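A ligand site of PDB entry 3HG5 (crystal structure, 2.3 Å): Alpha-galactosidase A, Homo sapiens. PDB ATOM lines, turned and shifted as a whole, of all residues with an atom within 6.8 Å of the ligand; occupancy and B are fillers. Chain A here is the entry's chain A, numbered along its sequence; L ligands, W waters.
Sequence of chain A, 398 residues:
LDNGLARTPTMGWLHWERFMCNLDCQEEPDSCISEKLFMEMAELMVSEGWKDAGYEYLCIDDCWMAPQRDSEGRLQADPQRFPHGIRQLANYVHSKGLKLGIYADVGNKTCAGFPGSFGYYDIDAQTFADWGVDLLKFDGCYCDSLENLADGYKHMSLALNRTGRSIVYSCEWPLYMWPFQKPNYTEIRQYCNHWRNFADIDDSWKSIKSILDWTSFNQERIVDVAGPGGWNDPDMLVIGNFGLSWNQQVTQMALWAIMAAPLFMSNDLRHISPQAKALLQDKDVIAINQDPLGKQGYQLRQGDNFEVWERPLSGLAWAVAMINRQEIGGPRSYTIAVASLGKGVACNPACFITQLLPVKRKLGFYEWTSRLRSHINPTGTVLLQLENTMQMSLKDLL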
ATOM      1  N   LEU A  14       2.800 -13.351 -23.950  1.00  0.00           N
ATOM      2  CA  LEU A  14       2.039 -13.490 -22.718  1.00  0.00           C
ATOM      3  C   LEU A  14       0.633 -13.904 -23.076  1.00  0.00           C
ATOM      4  O   LEU A  14       0.051 -13.327 -23.989  1.00  0.00           O
ATOM      5  CB  LEU A  14       2.054 -12.165 -21.958  1.00  0.00           C
ATOM      6  CG  LEU A  14       1.267 -12.020 -20.651  1.00  0.00           C
ATOM      7  CD1 LEU A  14       1.744 -13.019 -19.611  1.00  0.00           C
ATOM      8  CD2 LEU A  14       1.414 -10.587 -20.152  1.00  0.00           C
ATOM      9  N   TRP A  16      -2.436 -13.720 -21.733  1.00  0.00           N
ATOM     10  CA  TRP A  16      -3.694 -13.173 -21.203  1.00  0.00           C
ATOM     11  C   TRP A  16      -4.723 -12.693 -22.232  1.00  0.00           C
ATOM     12  O   TRP A  16      -5.854 -13.165 -22.233  1.00  0.00           O
ATOM     13  CB  TRP A  16      -3.484 -12.089 -20.145  1.00  0.00           C
ATOM     14  CG  TRP A  16      -4.804 -11.735 -19.499  1.00  0.00           C
ATOM     15  CD1 TRP A  16      -5.505 -10.577 -19.644  1.00  0.00           C
ATOM     16  CD2 TRP A  16      -5.615 -12.592 -18.661  1.00  0.00           C
ATOM     17  NE1 TRP A  16      -6.683 -10.630 -18.927  1.00  0.00           N
ATOM     18  CE2 TRP A  16      -6.782 -11.862 -18.330  1.00  0.00           C
ATOM     19  CE3 TRP A  16      -5.455 -13.896 -18.165  1.00  0.00           C
ATOM     20  CZ2 TRP A  16      -7.794 -12.400 -17.509  1.00  0.00           C
ATOM     21  CZ3 TRP A  16      -6.459 -14.423 -17.347  1.00  0.00           C
ATOM     22  CH2 TRP A  16      -7.618 -13.674 -17.025  1.00  0.00           C
ATOM     23  N   CYS A  21      -8.733 -16.752 -19.317  1.00  0.00           N
ATOM     24  CA  CYS A  21      -8.846 -17.772 -18.271  1.00  0.00           C
ATOM     25  C   CYS A  21      -9.693 -18.954 -18.757  1.00  0.00           C
ATOM     26  O   CYS A  21     -10.657 -19.366 -18.093  1.00  0.00           O
ATOM     27  CB  CYS A  21      -9.463 -17.156 -17.008  1.00  0.00           C
ATOM     28  SG  CYS A  21      -9.226 -18.158 -15.499  1.00  0.00           S
ATOM     29  N   ASP A  61       0.274 -16.181 -17.745  1.00  0.00           N
ATOM     30  CA  ASP A  61      -0.465 -15.191 -16.988  1.00  0.00           C
ATOM     31  C   ASP A  61      -1.325 -15.912 -15.939  1.00  0.00           C
ATOM     32  O   ASP A  61      -0.946 -16.995 -15.459  1.00  0.00           O
ATOM     33  CB  ASP A  61      -1.285 -14.300 -17.938  1.00  0.00           C
ATOM     34  CG  ASP A  61      -1.570 -12.918 -17.365  1.00  0.00           C
ATOM     35  OD1 ASP A  61      -2.466 -12.818 -16.505  1.00  0.00           O
ATOM     36  OD2 ASP A  61      -0.908 -11.944 -17.782  1.00  0.00           O
ATOM     37  N   ASP A  62      -2.472 -15.337 -15.580  1.00  0.00           N
ATOM     38  CA  ASP A  62      -3.357 -15.889 -14.543  1.00  0.00           C
ATOM     39  C   ASP A  62      -3.963 -17.231 -14.993  1.00  0.00           C
ATOM     40  O   ASP A  62      -3.968 -17.542 -16.186  1.00  0.00           O
ATOM     41  CB  ASP A  62      -4.473 -14.898 -14.245  1.00  0.00           C
ATOM     42  CG  ASP A  62      -5.058 -15.030 -12.834  1.00  0.00           C
ATOM     43  OD1 ASP A  62      -4.952 -16.104 -12.188  1.00  0.00           O
ATOM     44  OD2 ASP A  62      -5.646 -14.046 -12.369  1.00  0.00           O
ATOM     45  N   CYS A  63      -4.462 -18.001 -14.021  1.00  0.00           N
ATOM     46  CA  CYS A  63      -5.205 -19.246 -14.271  1.00  0.00           C
ATOM     47  C   CYS A  63      -4.320 -20.449 -14.630  1.00  0.00           C
ATOM     48  O   CYS A  63      -4.731 -21.328 -15.377  1.00  0.00           O
ATOM     49  CB  CYS A  63      -6.330 -19.030 -15.298  1.00  0.00           C
ATOM     50  SG  CYS A  63      -7.389 -17.606 -14.884  1.00  0.00           S
ATOM     51  N   TYR A 103       2.990 -15.819 -13.193  1.00  0.00           N
ATOM     52  CA  TYR A 103       2.098 -14.797 -12.647  1.00  0.00           C
ATOM     53  C   TYR A 103       1.730 -15.124 -11.192  1.00  0.00           C
ATOM     54  O   TYR A 103       1.464 -16.280 -10.846  1.00  0.00           O
ATOM     55  CB  TYR A 103       0.842 -14.686 -13.526  1.00  0.00           C
ATOM     56  CG  TYR A 103      -0.319 -13.877 -12.956  1.00  0.00           C
ATOM     57  CD1 TYR A 103      -0.605 -12.593 -13.415  1.00  0.00           C
ATOM     58  CD2 TYR A 103      -1.135 -14.415 -11.962  1.00  0.00           C
ATOM     59  CE1 TYR A 103      -1.667 -11.860 -12.893  1.00  0.00           C
ATOM     60  CE2 TYR A 103      -2.189 -13.684 -11.429  1.00  0.00           C
ATOM     61  CZ  TYR A 103      -2.449 -12.412 -11.900  1.00  0.00           C
ATOM     62  OH  TYR A 103      -3.504 -11.719 -11.349  1.00  0.00           O
ATOM     63  N   ASP A 105       0.035 -12.734  -7.407  1.00  0.00           N
ATOM     64  CA  ASP A 105      -0.736 -11.576  -6.978  1.00  0.00           C
ATOM     65  C   ASP A 105      -0.313 -11.179  -5.566  1.00  0.00           C
ATOM     66  O   ASP A 105      -0.052 -12.039  -4.714  1.00  0.00           O
ATOM     67  CB  ASP A 105      -2.238 -11.880  -7.065  1.00  0.00           C
ATOM     68  CG  ASP A 105      -3.103 -10.634  -6.978  1.00  0.00           C
ATOM     69  OD1 ASP A 105      -3.604 -10.201  -8.039  1.00  0.00           O
ATOM     70  OD2 ASP A 105      -3.302 -10.104  -5.874  1.00  0.00           O
ATOM     71  N   THR A 110      -5.529 -14.066  -6.668  1.00  0.00           N
ATOM     72  CA  THR A 110      -5.295 -13.514  -8.007  1.00  0.00           C
ATOM     73  C   THR A 110      -6.594 -12.888  -8.529  1.00  0.00           C
ATOM     74  O   THR A 110      -7.668 -13.131  -7.978  1.00  0.00           O
ATOM     75  CB  THR A 110      -4.767 -14.574  -8.995  1.00  0.00           C
ATOM     76  OG1 THR A 110      -5.801 -15.520  -9.310  1.00  0.00           O
ATOM     77  CG2 THR A 110      -3.550 -15.301  -8.434  1.00  0.00           C
ATOM     78  N   CYS A 111      -6.490 -12.090  -9.587  1.00  0.00           N
ATOM     79  CA  CYS A 111      -7.670 -11.441 -10.156  1.00  0.00           C
ATOM     80  C   CYS A 111      -8.698 -12.432 -10.676  1.00  0.00           C
ATOM     81  O   CYS A 111      -9.887 -12.130 -10.698  1.00  0.00           O
ATOM     82  CB  CYS A 111      -7.298 -10.439 -11.248  1.00  0.00           C
ATOM     83  SG  CYS A 111      -6.326  -9.040 -10.682  1.00  0.00           S
ATOM     84  N   ALA A 112      -8.256 -13.613 -11.099  1.00  0.00           N
ATOM     85  CA  ALA A 112      -9.188 -14.654 -11.512  1.00  0.00           C
ATOM     86  C   ALA A 112      -9.694 -15.515 -10.333  1.00  0.00           C
ATOM     87  O   ALA A 112     -10.576 -16.351 -10.507  1.00  0.00           O
ATOM     88  CB  ALA A 112      -8.582 -15.517 -12.583  1.00  0.00           C
ATOM     89  N   GLY A 113      -9.133 -15.289  -9.139  1.00  0.00           N
ATOM     90  CA  GLY A 113      -9.663 -15.909  -7.913  1.00  0.00           C
ATOM     91  C   GLY A 113      -8.883 -17.102  -7.387  1.00  0.00           C
ATOM     92  O   GLY A 113      -9.373 -17.840  -6.527  1.00  0.00           O
ATOM     93  N   LYS A 137       5.206 -11.787 -13.188  1.00  0.00           N
ATOM     94  CA  LYS A 137       4.204 -10.743 -13.264  1.00  0.00           C
ATOM     95  C   LYS A 137       3.398 -10.777 -11.969  1.00  0.00           C
ATOM     96  O   LYS A 137       2.757 -11.776 -11.648  1.00  0.00           O
ATOM     97  CB  LYS A 137       3.305 -10.906 -14.496  1.00  0.00           C
ATOM     98  CG  LYS A 137       2.293  -9.778 -14.701  1.00  0.00           C
ATOM     99  CD  LYS A 137       1.396 -10.034 -15.913  1.00  0.00           C
ATOM    100  CE  LYS A 137       0.191  -9.101 -15.933  1.00  0.00           C
ATOM    101  NZ  LYS A 137      -0.645  -9.303 -17.146  1.00  0.00           N
ATOM    102  N   ASP A 139       0.518  -9.121  -9.844  1.00  0.00           N
ATOM    103  CA  ASP A 139      -0.725  -8.356  -9.964  1.00  0.00           C
ATOM    104  C   ASP A 139      -1.177  -7.804  -8.610  1.00  0.00           C
ATOM    105  O   ASP A 139      -0.614  -8.152  -7.561  1.00  0.00           O
ATOM    106  CB  ASP A 139      -1.789  -9.278 -10.556  1.00  0.00           C
ATOM    107  CG  ASP A 139      -2.864  -8.530 -11.353  1.00  0.00           C
ATOM    108  OD1 ASP A 139      -2.982  -7.286 -11.251  1.00  0.00           O
ATOM    109  OD2 ASP A 139      -3.608  -9.217 -12.076  1.00  0.00           O
ATOM    110  N   GLY A 140      -2.216  -6.962  -8.622  1.00  0.00           N
ATOM    111  CA  GLY A 140      -2.632  -6.237  -7.433  1.00  0.00           C
ATOM    112  C   GLY A 140      -4.044  -6.428  -6.888  1.00  0.00           C
ATOM    113  O   GLY A 140      -4.465  -5.664  -6.032  1.00  0.00           O
ATOM    114  N   CYS A 141      -4.752  -7.458  -7.360  1.00  0.00           N
ATOM    115  CA  CYS A 141      -6.124  -7.734  -6.887  1.00  0.00           C
ATOM    116  C   CYS A 141      -6.211  -8.198  -5.443  1.00  0.00           C
ATOM    117  O   CYS A 141      -5.244  -8.727  -4.894  1.00  0.00           O
ATOM    118  CB  CYS A 141      -6.830  -8.754  -7.766  1.00  0.00           C
ATOM    119  SG  CYS A 141      -7.453  -8.095  -9.298  1.00  0.00           S
ATOM    120  N   GLU A 172       2.333  -4.347 -11.084  1.00  0.00           N
ATOM    121  CA  GLU A 172       1.116  -3.611 -11.436  1.00  0.00           C
ATOM    122  C   GLU A 172       0.797  -2.588 -10.370  1.00  0.00           C
ATOM    123  O   GLU A 172      -0.301  -2.047 -10.320  1.00  0.00           O
ATOM    124  CB  GLU A 172      -0.064  -4.576 -11.684  1.00  0.00           C
ATOM    125  CG  GLU A 172       0.204  -5.575 -12.797  1.00  0.00           C
ATOM    126  CD  GLU A 172      -1.059  -6.147 -13.417  1.00  0.00           C
ATOM    127  OE1 GLU A 172      -1.126  -7.392 -13.535  1.00  0.00           O
ATOM    128  OE2 GLU A 172      -1.956  -5.372 -13.798  1.00  0.00           O
ATOM    129  N   LEU A 175      -0.865   1.015 -11.146  1.00  0.00           N
ATOM    130  CA  LEU A 175      -2.254   0.810 -11.562  1.00  0.00           C
ATOM    131  C   LEU A 175      -3.250   0.719 -10.395  1.00  0.00           C
ATOM    132  O   LEU A 175      -4.328   1.322 -10.438  1.00  0.00           O
ATOM    133  CB  LEU A 175      -2.364  -0.444 -12.448  1.00  0.00           C
ATOM    134  CG  LEU A 175      -3.741  -0.981 -12.889  1.00  0.00           C
ATOM    135  CD1 LEU A 175      -4.466   0.005 -13.785  1.00  0.00           C
ATOM    136  CD2 LEU A 175      -3.584  -2.340 -13.598  1.00  0.00           C
ATOM    137  N   TYR A 176      -2.877  -0.030  -9.358  1.00  0.00           N
ATOM    138  CA  TYR A 176      -3.785  -0.256  -8.230  1.00  0.00           C
ATOM    139  C   TYR A 176      -3.780   0.852  -7.178  1.00  0.00           C
ATOM    140  O   TYR A 176      -4.716   0.955  -6.386  1.00  0.00           O
ATOM    141  CB  TYR A 176      -3.550  -1.633  -7.594  1.00  0.00           C
ATOM    142  CG  TYR A 176      -4.007  -2.745  -8.494  1.00  0.00           C
ATOM    143  CD1 TYR A 176      -5.334  -3.187  -8.479  1.00  0.00           C
ATOM    144  CD2 TYR A 176      -3.123  -3.328  -9.407  1.00  0.00           C
ATOM    145  CE1 TYR A 176      -5.754  -4.204  -9.338  1.00  0.00           C
ATOM    146  CE2 TYR A 176      -3.536  -4.340 -10.261  1.00  0.00           C
ATOM    147  CZ  TYR A 176      -4.846  -4.771 -10.220  1.00  0.00           C
ATOM    148  OH  TYR A 176      -5.243  -5.774 -11.066  1.00  0.00           O
ATOM    149  N   ARG A 196       2.850  -1.687 -14.788  1.00  0.00           N
ATOM    150  CA  ARG A 196       1.594  -1.427 -15.485  1.00  0.00           C
ATOM    151  C   ARG A 196       0.990  -0.165 -14.892  1.00  0.00           C
ATOM    152  O   ARG A 196       0.834  -0.053 -13.673  1.00  0.00           O
ATOM    153  CB  ARG A 196       0.630  -2.619 -15.350  1.00  0.00           C
ATOM    154  CG  ARG A 196       0.954  -3.830 -16.264  1.00  0.00           C
ATOM    155  CD  ARG A 196       0.361  -3.655 -17.706  1.00  0.00           C
ATOM    156  NE  ARG A 196      -1.017  -3.170 -17.655  1.00  0.00           N
ATOM    157  CZ  ARG A 196      -2.086  -3.931 -17.393  1.00  0.00           C
ATOM    158  NH1 ARG A 196      -1.945  -5.232 -17.196  1.00  0.00           N
ATOM    159  NH2 ARG A 196      -3.296  -3.383 -17.335  1.00  0.00           N
ATOM    160  N   PHE A 198      -1.915   1.534 -16.509  1.00  0.00           N
ATOM    161  CA  PHE A 198      -3.264   1.801 -17.013  1.00  0.00           C
ATOM    162  C   PHE A 198      -4.059   0.501 -17.232  1.00  0.00           C
ATOM    163  O   PHE A 198      -3.491  -0.597 -17.227  1.00  0.00           O
ATOM    164  CB  PHE A 198      -3.145   2.625 -18.316  1.00  0.00           C
ATOM    165  CG  PHE A 198      -4.444   3.225 -18.793  1.00  0.00           C
ATOM    166  CD1 PHE A 198      -5.068   4.260 -18.075  1.00  0.00           C
ATOM    167  CD2 PHE A 198      -5.031   2.794 -19.983  1.00  0.00           C
ATOM    168  CE1 PHE A 198      -6.267   4.841 -18.527  1.00  0.00           C
ATOM    169  CE2 PHE A 198      -6.245   3.360 -20.437  1.00  0.00           C
ATOM    170  CZ  PHE A 198      -6.854   4.389 -19.696  1.00  0.00           C
ATOM    171  N   ALA A 199      -5.372   0.660 -17.387  1.00  0.00           N
ATOM    172  CA  ALA A 199      -6.336  -0.434 -17.567  1.00  0.00           C
ATOM    173  C   ALA A 199      -5.894  -1.469 -18.588  1.00  0.00           C
ATOM    174  O   ALA A 199      -5.227  -1.150 -19.577  1.00  0.00           O
ATOM    175  CB  ALA A 199      -7.707   0.134 -17.934  1.00  0.00           C
ATOM    176  N   ASP A 200      -6.257  -2.732 -18.323  1.00  0.00           N
ATOM    177  CA  ASP A 200      -5.999  -3.849 -19.241  1.00  0.00           C
ATOM    178  C   ASP A 200      -6.327  -3.443 -20.674  1.00  0.00           C
ATOM    179  O   ASP A 200      -7.363  -2.837 -20.943  1.00  0.00           O
ATOM    180  CB  ASP A 200      -6.883  -5.045 -18.866  1.00  0.00           C
ATOM    181  CG  ASP A 200      -6.517  -5.671 -17.502  1.00  0.00           C
ATOM    182  OD1 ASP A 200      -5.628  -5.159 -16.786  1.00  0.00           O
ATOM    183  OD2 ASP A 200      -7.145  -6.702 -17.171  1.00  0.00           O
ATOM    184  N   ILE A 201      -5.436  -3.784 -21.596  1.00  0.00           N
ATOM    185  CA  ILE A 201      -5.716  -3.630 -23.016  1.00  0.00           C
ATOM    186  C   ILE A 201      -6.704  -4.720 -23.465  1.00  0.00           C
ATOM    187  O   ILE A 201      -6.779  -5.806 -22.874  1.00  0.00           O
ATOM    188  CB  ILE A 201      -4.420  -3.716 -23.861  1.00  0.00           C
ATOM    189  CG1 ILE A 201      -4.655  -3.189 -25.285  1.00  0.00           C
ATOM    190  CG2 ILE A 201      -3.860  -5.155 -23.861  1.00  0.00           C
ATOM    191  CD1 ILE A 201      -3.388  -2.834 -26.049  1.00  0.00           C
ATOM    192  N   ASP A 235       0.959  -2.129 -21.556  1.00  0.00           N
ATOM    193  CA  ASP A 235       0.314  -3.438 -21.755  1.00  0.00           C
ATOM    194  C   ASP A 235       0.702  -4.116 -23.097  1.00  0.00           C
ATOM    195  O   ASP A 235       1.502  -3.578 -23.890  1.00  0.00           O
ATOM    196  CB  ASP A 235      -1.211  -3.392 -21.555  1.00  0.00           C
ATOM    197  CG  ASP A 235      -1.765  -4.668 -20.917  1.00  0.00           C
ATOM    198  OD1 ASP A 235      -1.028  -5.675 -20.804  1.00  0.00           O
ATOM    199  OD2 ASP A 235      -2.943  -4.643 -20.494  1.00  0.00           O
ATOM    200  N   MET A 236       0.122  -5.295 -23.292  1.00  0.00           N
ATOM    201  CA  MET A 236       0.425  -6.219 -24.384  1.00  0.00           C
ATOM    202  C   MET A 236       0.221  -5.667 -25.796  1.00  0.00           C
ATOM    203  O   MET A 236      -0.698  -4.898 -26.070  1.00  0.00           O
ATOM    204  CB  MET A 236      -0.429  -7.496 -24.221  1.00  0.00           C
ATOM    205  CG  MET A 236      -0.060  -8.363 -23.018  1.00  0.00           C
ATOM    206  SD  MET A 236      -1.352  -9.558 -22.572  1.00  0.00           S
ATOM    207  CE  MET A 236      -2.498  -8.500 -21.702  1.00  0.00           C
HETATM  208  C1  LIG L   1      -5.392  -8.139 -14.184  1.00  0.00           C
HETATM  209  C2  LIG L   1      -4.185  -7.804 -15.070  1.00  0.00           C
HETATM  210  C3  LIG L   1      -4.364  -8.432 -16.448  1.00  0.00           C
HETATM  211  C4  LIG L   1      -4.436  -9.946 -16.254  1.00  0.00           C
HETATM  212  C5  LIG L   1      -5.555 -10.328 -15.273  1.00  0.00           C
HETATM  213  C6  LIG L   1      -5.431 -11.780 -14.858  1.00  0.00           C
HETATM  214  O1  LIG L   1      -6.615  -7.628 -14.724  1.00  0.00           O
HETATM  215  O2  LIG L   1      -3.963  -6.393 -15.154  1.00  0.00           O
HETATM  216  O3  LIG L   1      -3.288  -8.067 -17.317  1.00  0.00           O
HETATM  217  O4  LIG L   1      -3.169 -10.400 -15.756  1.00  0.00           O
HETATM  218  O5  LIG L   1      -5.534  -9.562 -14.070  1.00  0.00           O
HETATM  219  O6  LIG L   1      -6.575 -12.201 -14.104  1.00  0.00           O
HETATM  220  O   HOH W   1      -4.056  -6.793 -19.508  1.00  0.00           O
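OD1 of Asp 61 is in hydrogen-bond range of O4 of the ligand.
The side-chain carboxylate (OE2) of Glu 172 lies within hydrogen-bond range of an oxygen (O2) of the ligand, 2.6 Å away.
OD1 of Asp 200 lies within hydrogen-bond range of O2 of the ligand.
The side-chain carboxylate (OD2) of Asp 62 is in hydrogen-bond range of an oxygen (O6) of the ligand, at 2.7 Å.
O3 of the ligand is in hydrogen-bond range of NZ of Lys 137 (2.9 Å).
The guanidinium group (NH1) of Arg 196 sits at hydrogen-bond distance from an oxygen (O2) of the ligand.
The side-chain carboxylate (OE2) of Glu 172 lies within salt-bridge range of the guanidinium group (NH1) of Arg 196 (3.4 Å).
The side-chain carboxylate (OD2) of Asp 62 is in hydrogen-bond range of the side-chain hydroxyl (OH) of Tyr 103, at 3.3 Å.
The side-chain carboxylate (OD1) of Asp 62 is in hydrogen-bond range of the side-chain hydroxyl (OG1) of Thr 110, at 3.1 Å.
OD2 of Asp 139 sits at hydrogen-bond distance from OH of Tyr 103 (2.6 Å).
The guanidinium group of Arg 196 is in salt-bridge range of the side-chain carboxylate of Asp 235 (3.4 Å).
N of Cys 111 sits at hydrogen-bond distance from OH of Tyr 103 (3.5 Å).
SG of Cys 141 forms a disulfide with SG of Cys 111 (2.0 Å).
SG of Cys 63 is disulfide-bonded to SG of Cys 21 (2.0 Å).
SG of Cys 111 sits close to O5 of the ligand (3.5 Å).
The side-chain carboxylate of Asp 139 sits close to an oxygen (O5) of the ligand (2.8 Å).
Merely in contact with the ligand: Trp 16 (3.4 Å), Tyr 103 (3.5 Å), Ala 112 (3.7 Å) and Tyr 176 (3.9 Å).
Water W1 lies within hydrogen-bond range of OD2 of Asp 235 (2.6 Å), O3 of the ligand (2.6 Å) and NH1 of Arg 196 (3.5 Å).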
